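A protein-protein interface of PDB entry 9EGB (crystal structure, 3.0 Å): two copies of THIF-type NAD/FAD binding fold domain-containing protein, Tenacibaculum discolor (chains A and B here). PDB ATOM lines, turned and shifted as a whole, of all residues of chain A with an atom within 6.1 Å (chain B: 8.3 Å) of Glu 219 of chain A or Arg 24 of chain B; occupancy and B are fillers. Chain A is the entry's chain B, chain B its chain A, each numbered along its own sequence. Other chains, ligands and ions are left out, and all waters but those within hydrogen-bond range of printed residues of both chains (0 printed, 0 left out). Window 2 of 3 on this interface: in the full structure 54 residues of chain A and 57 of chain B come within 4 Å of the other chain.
Of the 13 printed residues of chain B, 5 touch a printed residue of chain A. Printed residues of chain B that touch a printed residue of chain A: Arg 22, Asn 23, Arg 24, Leu 25 and Tyr 26. Of the 15 printed residues of chain A, 7 touch a printed residue of chain B. Along chain A the printed residues that touch a printed residue of chain B span positions 212 to 227. Among the printed residues, Asp or Glu carboxylates within 4 Å of a Lys or Arg side-chain nitrogen of the other chain: Glu 219 of chain A with Arg 24 of chain B.
No position is printed for both chains. Of the 14 pairs that touch across the chains among the printed residues, none has its exchanged pair printed and touching as well.
Among the printed residues, merely in contact across the chains: Pro 226 of chain A with Arg 24 of chain B, Leu 223 of chain A with Arg 24 of chain B, Pro 226 of chain A with Arg 22 of chain B, Ile 212 of chain A with Tyr 26 of chain B, Ile 212 of chain A with Leu 25 of chain B, Pro 226 of chain A with Tyr 26 of chain B, Phe 216 of chain A with Leu 25 of chain B, Glu 219 of chain A with Leu 25 of chain B, Phe 216 of chain A with Arg 24 of chain B, Gln 227 of chain A with Asn 23 of chain B and Ser 224 of chain A with Arg 22 of chain B.
Of the printed residues of chain B, Glu 219 of chain A touches Arg 24 (2.8 Å) and Leu 25 (3.7 Å). Arg 24 of chain B touches five residues of chain A. Printed residues of chain A within 4 Å of Arg 22 of chain B: Ser 224, Pro 226 and Gln 227. Of the printed residues of chain B, Gln 227 of chain A touches Arg 22 and Asn 23. Of the printed residues of chain A, Asn 23 of chain B touches Gln 227. Glu 221 of chain A touches none of the printed residues of chain B. The nearest residue of chain B that does not touch Glu 219 of chain A is Ser 21 of chain B (7.8 Å). The nearest residue of chain A that does not touch Arg 24 of chain B is Pro 225 of chain A (4.4 Å).
O of Arg 22 of chain B is in hydrogen-bond range of N of Gln 227 of chain A, at 3.0 Å. NE of Arg 24 of chain B lies within salt-bridge range of OE2 of Glu 219 of chain A, 2.8 Å away. The backbone carbonyl oxygen (O) of Ser 224 of chain A is in hydrogen-bond range of the guanidinium group (NH2) of Arg 24 of chain B (2.7 Å).
ND2 of Asn 23 of chain B lies within hydrogen-bond range of OE1 of Gln 32 of chain B, at 2.8 Å.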
ATOM      1  N   ILE A 212     -27.212 -27.058 -29.328  1.00  0.00           N
ATOM      2  CA  ILE A 212     -26.730 -25.680 -29.254  1.00  0.00           C
ATOM      3  C   ILE A 212     -27.407 -24.796 -30.295  1.00  0.00           C
ATOM      4  O   ILE A 212     -27.675 -23.620 -30.025  1.00  0.00           O
ATOM      5  CB  ILE A 212     -25.191 -25.648 -29.400  1.00  0.00           C
ATOM      6  CG1 ILE A 212     -24.609 -24.296 -28.960  1.00  0.00           C
ATOM      7  CG2 ILE A 212     -24.742 -26.021 -30.803  1.00  0.00           C
ATOM      8  CD1 ILE A 212     -24.765 -23.997 -27.489  1.00  0.00           C
ATOM      9  N   TYR A 214     -30.550 -25.157 -31.284  1.00  0.00           N
ATOM     10  CA  TYR A 214     -31.857 -24.835 -30.718  1.00  0.00           C
ATOM     11  C   TYR A 214     -31.742 -23.754 -29.651  1.00  0.00           C
ATOM     12  O   TYR A 214     -32.456 -22.745 -29.691  1.00  0.00           O
ATOM     13  CB  TYR A 214     -32.525 -26.084 -30.127  1.00  0.00           C
ATOM     14  CG  TYR A 214     -33.943 -25.815 -29.625  1.00  0.00           C
ATOM     15  CD1 TYR A 214     -35.012 -25.693 -30.513  1.00  0.00           C
ATOM     16  CD2 TYR A 214     -34.201 -25.652 -28.266  1.00  0.00           C
ATOM     17  CE1 TYR A 214     -36.297 -25.434 -30.059  1.00  0.00           C
ATOM     18  CE2 TYR A 214     -35.484 -25.385 -27.804  1.00  0.00           C
ATOM     19  CZ  TYR A 214     -36.528 -25.276 -28.703  1.00  0.00           C
ATOM     20  OH  TYR A 214     -37.810 -25.013 -28.249  1.00  0.00           O
ATOM     21  N   LYS A 215     -30.804 -23.928 -28.717  1.00  0.00           N
ATOM     22  CA  LYS A 215     -30.606 -22.940 -27.663  1.00  0.00           C
ATOM     23  C   LYS A 215     -30.282 -21.575 -28.250  1.00  0.00           C
ATOM     24  O   LYS A 215     -30.776 -20.548 -27.768  1.00  0.00           O
ATOM     25  CB  LYS A 215     -29.492 -23.420 -26.731  1.00  0.00           C
ATOM     26  CG  LYS A 215     -29.885 -24.654 -25.918  1.00  0.00           C
ATOM     27  CD  LYS A 215     -30.051 -24.378 -24.450  1.00  0.00           C
ATOM     28  CE  LYS A 215     -28.770 -24.691 -23.700  1.00  0.00           C
ATOM     29  NZ  LYS A 215     -28.932 -24.433 -22.239  1.00  0.00           N
ATOM     30  N   PHE A 216     -29.422 -21.544 -29.267  1.00  0.00           N
ATOM     31  CA  PHE A 216     -29.006 -20.278 -29.861  1.00  0.00           C
ATOM     32  C   PHE A 216     -30.152 -19.598 -30.604  1.00  0.00           C
ATOM     33  O   PHE A 216     -30.307 -18.375 -30.518  1.00  0.00           O
ATOM     34  CB  PHE A 216     -27.809 -20.490 -30.782  1.00  0.00           C
ATOM     35  CG  PHE A 216     -27.361 -19.246 -31.493  1.00  0.00           C
ATOM     36  CD1 PHE A 216     -26.934 -18.142 -30.763  1.00  0.00           C
ATOM     37  CD2 PHE A 216     -27.303 -19.191 -32.870  1.00  0.00           C
ATOM     38  CE1 PHE A 216     -26.492 -16.998 -31.397  1.00  0.00           C
ATOM     39  CE2 PHE A 216     -26.861 -18.051 -33.506  1.00  0.00           C
ATOM     40  CZ  PHE A 216     -26.458 -16.951 -32.767  1.00  0.00           C
ATOM     41  N   LYS A 217     -30.932 -20.362 -31.389  1.00  0.00           N
ATOM     42  CA  LYS A 217     -32.029 -19.763 -32.157  1.00  0.00           C
ATOM     43  C   LYS A 217     -33.136 -19.221 -31.255  1.00  0.00           C
ATOM     44  O   LYS A 217     -33.650 -18.122 -31.491  1.00  0.00           O
ATOM     45  CB  LYS A 217     -32.600 -20.789 -33.142  1.00  0.00           C
ATOM     46  CG  LYS A 217     -31.616 -21.253 -34.211  1.00  0.00           C
ATOM     47  CD  LYS A 217     -32.306 -21.949 -35.393  1.00  0.00           C
ATOM     48  CE  LYS A 217     -33.222 -23.098 -34.955  1.00  0.00           C
ATOM     49  NZ  LYS A 217     -33.312 -24.198 -35.979  1.00  0.00           N
ATOM     50  N   ASN A 218     -33.498 -19.961 -30.205  1.00  0.00           N
ATOM     51  CA  ASN A 218     -34.514 -19.557 -29.236  1.00  0.00           C
ATOM     52  C   ASN A 218     -33.978 -18.634 -28.165  1.00  0.00           C
ATOM     53  O   ASN A 218     -34.624 -18.473 -27.121  1.00  0.00           O
ATOM     54  CB  ASN A 218     -35.184 -20.776 -28.600  1.00  0.00           C
ATOM     55  CG  ASN A 218     -36.065 -21.526 -29.572  1.00  0.00           C
ATOM     56  OD1 ASN A 218     -35.660 -22.531 -30.155  1.00  0.00           O
ATOM     57  ND2 ASN A 218     -37.296 -21.045 -29.740  1.00  0.00           N
ATOM     58  N   GLU A 219     -32.824 -18.020 -28.391  1.00  0.00           N
ATOM     59  CA  GLU A 219     -32.344 -16.999 -27.478  1.00  0.00           C
ATOM     60  C   GLU A 219     -33.254 -15.792 -27.601  1.00  0.00           C
ATOM     61  O   GLU A 219     -33.571 -15.356 -28.714  1.00  0.00           O
ATOM     62  CB  GLU A 219     -30.909 -16.607 -27.812  1.00  0.00           C
ATOM     63  CG  GLU A 219     -29.873 -17.102 -26.826  1.00  0.00           C
ATOM     64  CD  GLU A 219     -28.501 -16.517 -27.102  1.00  0.00           C
ATOM     65  OE1 GLU A 219     -28.290 -16.001 -28.227  1.00  0.00           O
ATOM     66  OE2 GLU A 219     -27.630 -16.599 -26.203  1.00  0.00           O
ATOM     67  N   ARG A 220     -33.674 -15.250 -26.455  1.00  0.00           N
ATOM     68  CA  ARG A 220     -34.523 -14.067 -26.472  1.00  0.00           C
ATOM     69  C   ARG A 220     -33.798 -12.928 -27.177  1.00  0.00           C
ATOM     70  O   ARG A 220     -34.283 -12.377 -28.172  1.00  0.00           O
ATOM     71  CB  ARG A 220     -34.868 -13.645 -25.036  1.00  0.00           C
ATOM     72  CG  ARG A 220     -35.658 -14.620 -24.144  1.00  0.00           C
ATOM     73  CD  ARG A 220     -36.778 -15.389 -24.818  1.00  0.00           C
ATOM     74  NE  ARG A 220     -37.274 -16.449 -23.936  1.00  0.00           N
ATOM     75  CZ  ARG A 220     -36.752 -17.672 -23.841  1.00  0.00           C
ATOM     76  NH1 ARG A 220     -35.697 -18.016 -24.572  1.00  0.00           N
ATOM     77  NH2 ARG A 220     -37.282 -18.554 -23.003  1.00  0.00           N
ATOM     78  N   GLU A 221     -32.630 -12.569 -26.663  1.00  0.00           N
ATOM     79  CA  GLU A 221     -31.783 -11.537 -27.234  1.00  0.00           C
ATOM     80  C   GLU A 221     -31.048 -12.055 -28.466  1.00  0.00           C
ATOM     81  O   GLU A 221     -30.789 -13.255 -28.605  1.00  0.00           O
ATOM     82  CB  GLU A 221     -30.791 -11.045 -26.191  1.00  0.00           C
ATOM     83  CG  GLU A 221     -31.480 -10.523 -24.952  1.00  0.00           C
ATOM     84  CD  GLU A 221     -30.508  -9.976 -23.937  1.00  0.00           C
ATOM     85  OE1 GLU A 221     -29.500 -10.660 -23.646  1.00  0.00           O
ATOM     86  OE2 GLU A 221     -30.756  -8.865 -23.427  1.00  0.00           O
ATOM     87  N   LYS A 222     -30.745 -11.136 -29.380  1.00  0.00           N
ATOM     88  CA  LYS A 222     -29.970 -11.429 -30.585  1.00  0.00           C
ATOM     89  C   LYS A 222     -28.500 -11.142 -30.267  1.00  0.00           C
ATOM     90  O   LYS A 222     -28.116  -9.985 -30.073  1.00  0.00           O
ATOM     91  CB  LYS A 222     -30.481 -10.596 -31.757  1.00  0.00           C
ATOM     92  CG  LYS A 222     -31.051  -9.259 -31.293  1.00  0.00           C
ATOM     93  CD  LYS A 222     -31.685  -8.440 -32.407  1.00  0.00           C
ATOM     94  CE  LYS A 222     -32.198  -7.119 -31.845  1.00  0.00           C
ATOM     95  NZ  LYS A 222     -32.713  -6.210 -32.898  1.00  0.00           N
ATOM     96  N   LEU A 223     -27.686 -12.196 -30.194  1.00  0.00           N
ATOM     97  CA  LEU A 223     -26.278 -12.129 -29.807  1.00  0.00           C
ATOM     98  C   LEU A 223     -25.415 -12.855 -30.827  1.00  0.00           C
ATOM     99  O   LEU A 223     -25.920 -13.470 -31.766  1.00  0.00           O
ATOM    100  CB  LEU A 223     -26.047 -12.720 -28.410  1.00  0.00           C
ATOM    101  CG  LEU A 223     -26.809 -12.070 -27.265  1.00  0.00           C
ATOM    102  CD1 LEU A 223     -26.699 -12.883 -26.013  1.00  0.00           C
ATOM    103  CD2 LEU A 223     -26.197 -10.718 -27.025  1.00  0.00           C
ATOM    104  N   SER A 224     -24.092 -12.695 -30.676  1.00  0.00           N
ATOM    105  CA  SER A 224     -23.125 -13.444 -31.473  1.00  0.00           C
ATOM    106  C   SER A 224     -23.099 -14.921 -31.052  1.00  0.00           C
ATOM    107  O   SER A 224     -23.330 -15.247 -29.883  1.00  0.00           O
ATOM    108  CB  SER A 224     -21.728 -12.839 -31.321  1.00  0.00           C
ATOM    109  OG  SER A 224     -21.728 -11.434 -31.528  1.00  0.00           O
ATOM    110  N   PRO A 225     -22.779 -15.829 -31.976  1.00  0.00           N
ATOM    111  CA  PRO A 225     -22.740 -17.247 -31.637  1.00  0.00           C
ATOM    112  C   PRO A 225     -21.690 -17.538 -30.587  1.00  0.00           C
ATOM    113  O   PRO A 225     -20.603 -16.939 -30.595  1.00  0.00           O
ATOM    114  CB  PRO A 225     -22.362 -17.919 -32.963  1.00  0.00           C
ATOM    115  CG  PRO A 225     -22.662 -16.948 -34.008  1.00  0.00           C
ATOM    116  CD  PRO A 225     -22.454 -15.601 -33.392  1.00  0.00           C
ATOM    117  N   PRO A 226     -21.978 -18.445 -29.664  1.00  0.00           N
ATOM    118  CA  PRO A 226     -20.944 -18.867 -28.721  1.00  0.00           C
ATOM    119  C   PRO A 226     -19.885 -19.693 -29.436  1.00  0.00           C
ATOM    120  O   PRO A 226     -20.154 -20.401 -30.409  1.00  0.00           O
ATOM    121  CB  PRO A 226     -21.716 -19.697 -27.692  1.00  0.00           C
ATOM    122  CG  PRO A 226     -22.913 -20.208 -28.456  1.00  0.00           C
ATOM    123  CD  PRO A 226     -23.270 -19.113 -29.422  1.00  0.00           C
ATOM    124  N   GLN A 227     -18.669 -19.631 -28.915  1.00  0.00           N
ATOM    125  CA  GLN A 227     -17.584 -20.443 -29.433  1.00  0.00           C
ATOM    126  C   GLN A 227     -16.706 -20.809 -28.243  1.00  0.00           C
ATOM    127  O   GLN A 227     -16.573 -20.035 -27.287  1.00  0.00           O
ATOM    128  CB  GLN A 227     -16.792 -19.707 -30.520  1.00  0.00           C
ATOM    129  CG  GLN A 227     -17.618 -19.025 -31.590  1.00  0.00           C
ATOM    130  CD  GLN A 227     -16.762 -18.370 -32.663  1.00  0.00           C
ATOM    131  OE1 GLN A 227     -15.531 -18.463 -32.633  1.00  0.00           O
ATOM    132  NE2 GLN A 227     -17.410 -17.712 -33.625  1.00  0.00           N
ATOM    133  N   MET B  16     -21.447 -14.497 -16.366  1.00  0.00           N
ATOM    134  CA  MET B  16     -20.065 -14.895 -16.631  1.00  0.00           C
ATOM    135  C   MET B  16     -19.217 -13.643 -16.881  1.00  0.00           C
ATOM    136  O   MET B  16     -19.774 -12.568 -17.129  1.00  0.00           O
ATOM    137  CB  MET B  16     -20.019 -15.868 -17.814  1.00  0.00           C
ATOM    138  CG  MET B  16     -20.921 -17.084 -17.592  1.00  0.00           C
ATOM    139  SD  MET B  16     -21.454 -17.977 -19.065  1.00  0.00           S
ATOM    140  CE  MET B  16     -20.014 -18.975 -19.414  1.00  0.00           C
ATOM    141  N   LYS B  17     -17.888 -13.755 -16.791  1.00  0.00           N
ATOM    142  CA  LYS B  17     -17.073 -12.554 -16.915  1.00  0.00           C
ATOM    143  C   LYS B  17     -16.930 -12.191 -18.394  1.00  0.00           C
ATOM    144  O   LYS B  17     -17.160 -13.025 -19.278  1.00  0.00           O
ATOM    145  CB  LYS B  17     -15.718 -12.820 -16.263  1.00  0.00           C
ATOM    146  CG  LYS B  17     -15.821 -13.033 -14.755  1.00  0.00           C
ATOM    147  CD  LYS B  17     -14.465 -13.222 -14.117  1.00  0.00           C
ATOM    148  CE  LYS B  17     -14.135 -14.715 -14.159  1.00  0.00           C
ATOM    149  NZ  LYS B  17     -12.814 -15.069 -13.593  1.00  0.00           N
ATOM    150  N   TYR B  20     -15.129 -14.675 -20.547  1.00  0.00           N
ATOM    151  CA  TYR B  20     -15.858 -15.895 -20.868  1.00  0.00           C
ATOM    152  C   TYR B  20     -17.222 -15.629 -21.495  1.00  0.00           C
ATOM    153  O   TYR B  20     -18.095 -16.502 -21.448  1.00  0.00           O
ATOM    154  CB  TYR B  20     -16.004 -16.740 -19.598  1.00  0.00           C
ATOM    155  CG  TYR B  20     -14.661 -17.060 -18.962  1.00  0.00           C
ATOM    156  CD1 TYR B  20     -13.693 -17.783 -19.646  1.00  0.00           C
ATOM    157  CD2 TYR B  20     -14.353 -16.601 -17.685  1.00  0.00           C
ATOM    158  CE1 TYR B  20     -12.463 -18.049 -19.074  1.00  0.00           C
ATOM    159  CE2 TYR B  20     -13.123 -16.870 -17.102  1.00  0.00           C
ATOM    160  CZ  TYR B  20     -12.184 -17.593 -17.804  1.00  0.00           C
ATOM    161  OH  TYR B  20     -10.959 -17.856 -17.239  1.00  0.00           O
ATOM    162  N   SER B  21     -17.422 -14.442 -22.073  1.00  0.00           N
ATOM    163  CA  SER B  21     -18.726 -14.087 -22.625  1.00  0.00           C
ATOM    164  C   SER B  21     -19.172 -15.097 -23.673  1.00  0.00           C
ATOM    165  O   SER B  21     -20.303 -15.595 -23.633  1.00  0.00           O
ATOM    166  CB  SER B  21     -18.669 -12.684 -23.216  1.00  0.00           C
ATOM    167  OG  SER B  21     -19.789 -12.451 -24.044  1.00  0.00           O
ATOM    168  N   ARG B  22     -18.293 -15.431 -24.610  1.00  0.00           N
ATOM    169  CA  ARG B  22     -18.673 -16.339 -25.684  1.00  0.00           C
ATOM    170  C   ARG B  22     -18.701 -17.803 -25.255  1.00  0.00           C
ATOM    171  O   ARG B  22     -18.940 -18.670 -26.099  1.00  0.00           O
ATOM    172  CB  ARG B  22     -17.707 -16.193 -26.850  1.00  0.00           C
ATOM    173  CG  ARG B  22     -17.601 -14.812 -27.407  1.00  0.00           C
ATOM    174  CD  ARG B  22     -18.884 -14.364 -28.038  1.00  0.00           C
ATOM    175  NE  ARG B  22     -18.566 -13.483 -29.151  1.00  0.00           N
ATOM    176  CZ  ARG B  22     -18.439 -12.170 -29.036  1.00  0.00           C
ATOM    177  NH1 ARG B  22     -18.615 -11.591 -27.857  1.00  0.00           N
ATOM    178  NH2 ARG B  22     -18.135 -11.440 -30.098  1.00  0.00           N
ATOM    179  N   ASN B  23     -18.480 -18.099 -23.976  1.00  0.00           N
ATOM    180  CA  ASN B  23     -18.639 -19.452 -23.464  1.00  0.00           C
ATOM    181  C   ASN B  23     -20.093 -19.790 -23.177  1.00  0.00           C
ATOM    182  O   ASN B  23     -20.377 -20.929 -22.792  1.00  0.00           O
ATOM    183  CB  ASN B  23     -17.822 -19.652 -22.179  1.00  0.00           C
ATOM    184  CG  ASN B  23     -16.412 -20.184 -22.431  1.00  0.00           C
ATOM    185  OD1 ASN B  23     -15.907 -20.195 -23.563  1.00  0.00           O
ATOM    186  ND2 ASN B  23     -15.771 -20.646 -21.354  1.00  0.00           N
ATOM    187  N   ARG B  24     -21.004 -18.825 -23.324  1.00  0.00           N
ATOM    188  CA  ARG B  24     -22.391 -18.992 -22.905  1.00  0.00           C
ATOM    189  C   ARG B  24     -23.103 -20.063 -23.736  1.00  0.00           C
ATOM    190  O   ARG B  24     -22.646 -20.473 -24.809  1.00  0.00           O
ATOM    191  CB  ARG B  24     -23.146 -17.676 -23.026  1.00  0.00           C
ATOM    192  CG  ARG B  24     -23.282 -17.200 -24.441  1.00  0.00           C
ATOM    193  CD  ARG B  24     -24.199 -15.986 -24.533  1.00  0.00           C
ATOM    194  NE  ARG B  24     -24.971 -16.026 -25.766  1.00  0.00           N
ATOM    195  CZ  ARG B  24     -24.473 -15.739 -26.963  1.00  0.00           C
ATOM    196  NH1 ARG B  24     -23.201 -15.379 -27.088  1.00  0.00           N
ATOM    197  NH2 ARG B  24     -25.247 -15.814 -28.036  1.00  0.00           N
ATOM    198  N   LEU B  25     -24.254 -20.503 -23.219  1.00  0.00           N
ATOM    199  CA  LEU B  25     -25.033 -21.611 -23.771  1.00  0.00           C
ATOM    200  C   LEU B  25     -24.286 -22.930 -23.612  1.00  0.00           C
ATOM    201  O   LEU B  25     -24.856 -23.901 -23.102  1.00  0.00           O
ATOM    202  CB  LEU B  25     -25.422 -21.378 -25.231  1.00  0.00           C
ATOM    203  CG  LEU B  25     -26.265 -20.140 -25.523  1.00  0.00           C
ATOM    204  CD1 LEU B  25     -26.706 -20.142 -26.976  1.00  0.00           C
ATOM    205  CD2 LEU B  25     -27.464 -20.159 -24.615  1.00  0.00           C
ATOM    206  N   TYR B  26     -23.025 -22.988 -24.054  1.00  0.00           N
ATOM    207  CA  TYR B  26     -22.213 -24.181 -23.814  1.00  0.00           C
ATOM    208  C   TYR B  26     -21.986 -24.407 -22.323  1.00  0.00           C
ATOM    209  O   TYR B  26     -22.058 -25.543 -21.841  1.00  0.00           O
ATOM    210  CB  TYR B  26     -20.874 -24.082 -24.545  1.00  0.00           C
ATOM    211  CG  TYR B  26     -20.985 -24.171 -26.045  1.00  0.00           C
ATOM    212  CD1 TYR B  26     -21.397 -25.341 -26.659  1.00  0.00           C
ATOM    213  CD2 TYR B  26     -20.650 -23.093 -26.849  1.00  0.00           C
ATOM    214  CE1 TYR B  26     -21.488 -25.433 -28.041  1.00  0.00           C
ATOM    215  CE2 TYR B  26     -20.738 -23.172 -28.227  1.00  0.00           C
ATOM    216  CZ  TYR B  26     -21.159 -24.345 -28.821  1.00  0.00           C
ATOM    217  OH  TYR B  26     -21.246 -24.427 -30.199  1.00  0.00           O
ATOM    218  N   LEU B  27     -21.680 -23.345 -21.585  1.00  0.00           N
ATOM    219  CA  LEU B  27     -21.493 -23.418 -20.142  1.00  0.00           C
ATOM    220  C   LEU B  27     -22.420 -22.418 -19.466  1.00  0.00           C
ATOM    221  O   LEU B  27     -22.570 -21.284 -19.935  1.00  0.00           O
ATOM    222  CB  LEU B  27     -20.055 -23.100 -19.725  1.00  0.00           C
ATOM    223  CG  LEU B  27     -18.932 -24.099 -19.975  1.00  0.00           C
ATOM    224  CD1 LEU B  27     -18.561 -24.114 -21.450  1.00  0.00           C
ATOM    225  CD2 LEU B  27     -17.740 -23.759 -19.103  1.00  0.00           C
ATOM    226  N   ASN B  28     -23.021 -22.825 -18.360  1.00  0.00           N
ATOM    227  CA  ASN B  28     -23.784 -21.895 -17.540  1.00  0.00           C
ATOM    228  C   ASN B  28     -22.859 -21.201 -16.549  1.00  0.00           C
ATOM    229  O   ASN B  28     -21.719 -21.625 -16.339  1.00  0.00           O
ATOM    230  CB  ASN B  28     -24.928 -22.638 -16.851  1.00  0.00           C
ATOM    231  CG  ASN B  28     -24.449 -23.700 -15.897  1.00  0.00           C
ATOM    232  OD1 ASN B  28     -23.814 -23.415 -14.883  1.00  0.00           O
ATOM    233  ND2 ASN B  28     -24.762 -24.945 -16.216  1.00  0.00           N
ATOM    234  N   PRO B  29     -23.319 -20.107 -15.922  1.00  0.00           N
ATOM    235  CA  PRO B  29     -22.439 -19.387 -14.983  1.00  0.00           C
ATOM    236  C   PRO B  29     -21.875 -20.247 -13.868  1.00  0.00           C
ATOM    237  O   PRO B  29     -20.719 -20.056 -13.465  1.00  0.00           O
ATOM    238  CB  PRO B  29     -23.363 -18.303 -14.418  1.00  0.00           C
ATOM    239  CG  PRO B  29     -24.312 -18.034 -15.506  1.00  0.00           C
ATOM    240  CD  PRO B  29     -24.569 -19.364 -16.167  1.00  0.00           C
ATOM    241  N   GLN B  32     -18.896 -22.372 -15.165  1.00  0.00           N
ATOM    242  CA  GLN B  32     -17.709 -21.531 -15.304  1.00  0.00           C
ATOM    243  C   GLN B  32     -17.055 -21.274 -13.956  1.00  0.00           C
ATOM    244  O   GLN B  32     -15.822 -21.292 -13.842  1.00  0.00           O
ATOM    245  CB  GLN B  32     -18.064 -20.222 -16.018  1.00  0.00           C
ATOM    246  CG  GLN B  32     -16.837 -19.435 -16.461  1.00  0.00           C
ATOM    247  CD  GLN B  32     -16.095 -20.060 -17.629  1.00  0.00           C
ATOM    248  OE1 GLN B  32     -16.614 -20.185 -18.740  1.00  0.00           O
ATOM    249  NE2 GLN B  32     -14.850 -20.450 -17.372  1.00  0.00           N
